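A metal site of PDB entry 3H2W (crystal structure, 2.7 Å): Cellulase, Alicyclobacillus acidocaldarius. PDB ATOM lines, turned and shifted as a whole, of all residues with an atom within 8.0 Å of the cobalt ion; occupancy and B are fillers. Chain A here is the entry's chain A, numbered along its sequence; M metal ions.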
ATOM      1  N   PRO A 115      26.614 -16.480  -1.350  1.00  0.00           N
ATOM      2  CA  PRO A 115      27.769 -17.267  -0.912  1.00  0.00           C
ATOM      3  C   PRO A 115      27.464 -18.359   0.102  1.00  0.00           C
ATOM      4  O   PRO A 115      28.328 -19.198   0.348  1.00  0.00           O
ATOM      5  CB  PRO A 115      28.708 -16.219  -0.288  1.00  0.00           C
ATOM      6  CG  PRO A 115      28.213 -14.906  -0.762  1.00  0.00           C
ATOM      7  CD  PRO A 115      26.754 -15.053  -0.983  1.00  0.00           C
ATOM      8  N   TRP A 116      26.269 -18.340   0.687  1.00  0.00           N
ATOM      9  CA  TRP A 116      25.885 -19.326   1.704  1.00  0.00           C
ATOM     10  C   TRP A 116      24.973 -20.383   1.125  1.00  0.00           C
ATOM     11  O   TRP A 116      24.216 -21.011   1.848  1.00  0.00           O
ATOM     12  CB  TRP A 116      25.196 -18.634   2.892  1.00  0.00           C
ATOM     13  CG  TRP A 116      25.995 -17.504   3.385  1.00  0.00           C
ATOM     14  CD1 TRP A 116      27.094 -17.563   4.189  1.00  0.00           C
ATOM     15  CD2 TRP A 116      25.818 -16.139   3.036  1.00  0.00           C
ATOM     16  NE1 TRP A 116      27.605 -16.308   4.367  1.00  0.00           N
ATOM     17  CE2 TRP A 116      26.836 -15.418   3.670  1.00  0.00           C
ATOM     18  CE3 TRP A 116      24.905 -15.464   2.251  1.00  0.00           C
ATOM     19  CZ2 TRP A 116      26.954 -14.044   3.554  1.00  0.00           C
ATOM     20  CZ3 TRP A 116      25.017 -14.097   2.123  1.00  0.00           C
ATOM     21  CH2 TRP A 116      26.036 -13.396   2.778  1.00  0.00           C
ATOM     22  N   ARG A 458      29.941 -11.529  14.182  1.00  0.00           N
ATOM     23  CA  ARG A 458      30.900 -12.017  13.178  1.00  0.00           C
ATOM     24  C   ARG A 458      31.171 -13.502  13.222  1.00  0.00           C
ATOM     25  O   ARG A 458      31.445 -14.103  12.193  1.00  0.00           O
ATOM     26  CB  ARG A 458      32.244 -11.328  13.369  1.00  0.00           C
ATOM     27  CG  ARG A 458      32.159  -9.846  13.475  1.00  0.00           C
ATOM     28  CD  ARG A 458      32.209  -9.192  12.140  1.00  0.00           C
ATOM     29  NE  ARG A 458      33.569  -8.772  11.858  1.00  0.00           N
ATOM     30  CZ  ARG A 458      33.976  -7.507  11.770  1.00  0.00           C
ATOM     31  NH1 ARG A 458      33.140  -6.480  11.925  1.00  0.00           N
ATOM     32  NH2 ARG A 458      35.265  -7.273  11.507  1.00  0.00           N
ATOM     33  N   PRO A 460      29.214 -16.388  14.783  1.00  0.00           N
ATOM     34  CA  PRO A 460      28.138 -17.103  15.473  1.00  0.00           C
ATOM     35  C   PRO A 460      28.421 -18.610  15.632  1.00  0.00           C
ATOM     36  O   PRO A 460      29.097 -19.210  14.796  1.00  0.00           O
ATOM     37  CB  PRO A 460      26.940 -16.886  14.545  1.00  0.00           C
ATOM     38  CG  PRO A 460      27.531 -16.654  13.192  1.00  0.00           C
ATOM     39  CD  PRO A 460      28.791 -15.901  13.467  1.00  0.00           C
ATOM     40  N   HIS A 462      27.170 -21.269  14.629  1.00  0.00           N
ATOM     41  CA  HIS A 462      26.290 -21.681  13.549  1.00  0.00           C
ATOM     42  C   HIS A 462      27.141 -22.522  12.609  1.00  0.00           C
ATOM     43  O   HIS A 462      28.009 -21.989  11.940  1.00  0.00           O
ATOM     44  CB  HIS A 462      25.747 -20.434  12.851  1.00  0.00           C
ATOM     45  CG  HIS A 462      24.838 -20.702  11.692  1.00  0.00           C
ATOM     46  ND1 HIS A 462      23.627 -21.354  11.824  1.00  0.00           N
ATOM     47  CD2 HIS A 462      24.937 -20.358  10.381  1.00  0.00           C
ATOM     48  CE1 HIS A 462      23.035 -21.413  10.644  1.00  0.00           C
ATOM     49  NE2 HIS A 462      23.815 -20.836   9.753  1.00  0.00           N
ATOM     50  N   ARG A 463      26.886 -23.828  12.575  1.00  0.00           N
ATOM     51  CA  ARG A 463      27.736 -24.790  11.840  1.00  0.00           C
ATOM     52  C   ARG A 463      27.962 -24.463  10.362  1.00  0.00           C
ATOM     53  O   ARG A 463      29.067 -24.652   9.832  1.00  0.00           O
ATOM     54  CB  ARG A 463      27.222 -26.224  11.990  1.00  0.00           C
ATOM     55  CG  ARG A 463      27.829 -26.960  13.194  1.00  0.00           C
ATOM     56  CD  ARG A 463      27.017 -28.192  13.577  1.00  0.00           C
ATOM     57  NE  ARG A 463      27.463 -28.830  14.828  1.00  0.00           N
ATOM     58  CZ  ARG A 463      27.186 -28.393  16.052  1.00  0.00           C
ATOM     59  NH1 ARG A 463      26.507 -27.280  16.257  1.00  0.00           N
ATOM     60  NH2 ARG A 463      27.620 -29.065  17.097  1.00  0.00           N
ATOM     61  N   PRO A 464      26.908 -24.018   9.674  1.00  0.00           N
ATOM     62  CA  PRO A 464      27.082 -23.530   8.305  1.00  0.00           C
ATOM     63  C   PRO A 464      28.036 -22.332   8.165  1.00  0.00           C
ATOM     64  O   PRO A 464      28.836 -22.296   7.235  1.00  0.00           O
ATOM     65  CB  PRO A 464      25.662 -23.155   7.891  1.00  0.00           C
ATOM     66  CG  PRO A 464      24.800 -24.044   8.739  1.00  0.00           C
ATOM     67  CD  PRO A 464      25.487 -24.050  10.061  1.00  0.00           C
ATOM     68  N   SER A 465      27.952 -21.371   9.085  1.00  0.00           N
ATOM     69  CA  SER A 465      28.773 -20.176   9.031  1.00  0.00           C
ATOM     70  C   SER A 465      30.201 -20.523   9.343  1.00  0.00           C
ATOM     71  O   SER A 465      31.118 -19.910   8.826  1.00  0.00           O
ATOM     72  CB  SER A 465      28.275 -19.138  10.028  1.00  0.00           C
ATOM     73  OG  SER A 465      27.203 -18.379   9.486  1.00  0.00           O
ATOM     74  N   VAL A 466      30.356 -21.540  10.194  1.00  0.00           N
ATOM     75  CA  VAL A 466      31.650 -22.068  10.554  1.00  0.00           C
ATOM     76  C   VAL A 466      32.237 -22.971   9.460  1.00  0.00           C
ATOM     77  O   VAL A 466      33.419 -22.849   9.145  1.00  0.00           O
ATOM     78  CB  VAL A 466      31.610 -22.800  11.912  1.00  0.00           C
ATOM     79  CG1 VAL A 466      32.824 -23.662  12.097  1.00  0.00           C
ATOM     80  CG2 VAL A 466      31.501 -21.781  13.050  1.00  0.00           C
ATOM     81  N   ALA A 467      31.422 -23.845   8.868  1.00  0.00           N
ATOM     82  CA  ALA A 467      31.961 -24.908   7.981  1.00  0.00           C
ATOM     83  C   ALA A 467      32.126 -24.498   6.519  1.00  0.00           C
ATOM     84  O   ALA A 467      33.010 -25.031   5.827  1.00  0.00           O
ATOM     85  CB  ALA A 467      31.144 -26.196   8.088  1.00  0.00           C
ATOM     86  N   ASP A 468      31.276 -23.588   6.019  1.00  0.00           N
ATOM     87  CA  ASP A 468      31.501 -22.999   4.690  1.00  0.00           C
ATOM     88  C   ASP A 468      32.832 -22.280   4.816  1.00  0.00           C
ATOM     89  O   ASP A 468      33.386 -22.224   5.927  1.00  0.00           O
ATOM     90  CB  ASP A 468      30.354 -22.057   4.273  1.00  0.00           C
ATOM     91  CG  ASP A 468      30.270 -20.769   5.116  1.00  0.00           C
ATOM     92  OD1 ASP A 468      31.291 -20.310   5.663  1.00  0.00           O
ATOM     93  OD2 ASP A 468      29.177 -20.188   5.215  1.00  0.00           O
ATOM     94  N   ASP A 469      33.390 -21.762   3.739  1.00  0.00           N
ATOM     95  CA  ASP A 469      34.621 -20.971   3.925  1.00  0.00           C
ATOM     96  C   ASP A 469      34.360 -19.635   3.304  1.00  0.00           C
ATOM     97  O   ASP A 469      34.929 -19.260   2.261  1.00  0.00           O
ATOM     98  CB  ASP A 469      35.863 -21.676   3.400  1.00  0.00           C
ATOM     99  CG  ASP A 469      36.340 -22.777   4.337  1.00  0.00           C
ATOM    100  OD1 ASP A 469      35.784 -23.887   4.300  1.00  0.00           O
ATOM    101  OD2 ASP A 469      37.266 -22.523   5.122  1.00  0.00           O
ATOM    102  N   VAL A 470      33.423 -18.977   3.984  1.00  0.00           N
ATOM    103  CA  VAL A 470      33.007 -17.608   3.750  1.00  0.00           C
ATOM    104  C   VAL A 470      33.165 -16.866   5.098  1.00  0.00           C
ATOM    105  O   VAL A 470      32.611 -17.328   6.104  1.00  0.00           O
ATOM    106  CB  VAL A 470      31.523 -17.581   3.297  1.00  0.00           C
ATOM    107  CG1 VAL A 470      31.095 -16.182   2.917  1.00  0.00           C
ATOM    108  CG2 VAL A 470      31.276 -18.578   2.169  1.00  0.00           C
ATOM    109  N   ASP A 471      33.919 -15.766   5.123  1.00  0.00           N
ATOM    110  CA  ASP A 471      34.190 -15.048   6.403  1.00  0.00           C
ATOM    111  C   ASP A 471      32.905 -14.631   7.057  1.00  0.00           C
ATOM    112  O   ASP A 471      32.563 -15.117   8.116  1.00  0.00           O
ATOM    113  CB  ASP A 471      35.054 -13.807   6.194  1.00  0.00           C
ATOM    114  CG  ASP A 471      36.405 -14.145   5.675  1.00  0.00           C
ATOM    115  OD1 ASP A 471      36.801 -15.328   5.801  1.00  0.00           O
ATOM    116  OD2 ASP A 471      37.072 -13.247   5.114  1.00  0.00           O
ATOM    117  N   HIS A 472      32.193 -13.760   6.361  1.00  0.00           N
ATOM    118  CA  HIS A 472      30.906 -13.293   6.799  1.00  0.00           C
ATOM    119  C   HIS A 472      29.975 -14.493   7.035  1.00  0.00           C
ATOM    120  O   HIS A 472      29.903 -15.406   6.227  1.00  0.00           O
ATOM    121  CB  HIS A 472      30.313 -12.317   5.769  1.00  0.00           C
ATOM    122  CG  HIS A 472      31.029 -11.000   5.713  1.00  0.00           C
ATOM    123  ND1 HIS A 472      32.395 -10.873   5.884  1.00  0.00           N
ATOM    124  CD2 HIS A 472      30.569  -9.747   5.471  1.00  0.00           C
ATOM    125  CE1 HIS A 472      32.748  -9.604   5.776  1.00  0.00           C
ATOM    126  NE2 HIS A 472      31.657  -8.902   5.526  1.00  0.00           N
ATOM    127  N   PRO A 473      29.294 -14.511   8.174  1.00  0.00           N
ATOM    128  CA  PRO A 473      28.322 -15.553   8.461  1.00  0.00           C
ATOM    129  C   PRO A 473      27.019 -15.313   7.705  1.00  0.00           C
ATOM    130  O   PRO A 473      26.817 -14.223   7.191  1.00  0.00           O
ATOM    131  CB  PRO A 473      28.099 -15.390   9.954  1.00  0.00           C
ATOM    132  CG  PRO A 473      28.303 -13.918  10.200  1.00  0.00           C
ATOM    133  CD  PRO A 473      29.410 -13.546   9.286  1.00  0.00           C
ATOM    134  N   VAL A 474      26.140 -16.311   7.663  1.00  0.00           N
ATOM    135  CA  VAL A 474      24.789 -16.140   7.113  1.00  0.00           C
ATOM    136  C   VAL A 474      24.241 -14.876   7.772  1.00  0.00           C
ATOM    137  O   VAL A 474      24.311 -14.744   8.978  1.00  0.00           O
ATOM    138  CB  VAL A 474      23.883 -17.399   7.416  1.00  0.00           C
ATOM    139  CG1 VAL A 474      22.464 -17.229   6.883  1.00  0.00           C
ATOM    140  CG2 VAL A 474      24.503 -18.676   6.864  1.00  0.00           C
HETATM  141 CO    CO M   1      31.776 -18.887   7.252  1.00  0.00          CO
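The side-chain hydroxyl (OG) of Ser 465 lies within hydrogen-bond range of the backbone NH (N) of Val 474, 3.0 Å away.
Asp 471 touches the cobalt ion (O to CO, 3.9 Å). Within 4 Å of the cobalt ion: Ser 465, Asp 468, Val 470 and Asp 471.
The cobalt ion is bound by the backbone carbonyl oxygen of Ser 465 (2.0 Å), the backbone carbonyl oxygen of Val 470 (2.1 Å) and the side-chain carboxylate of Asp 468 (2.2 Å).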
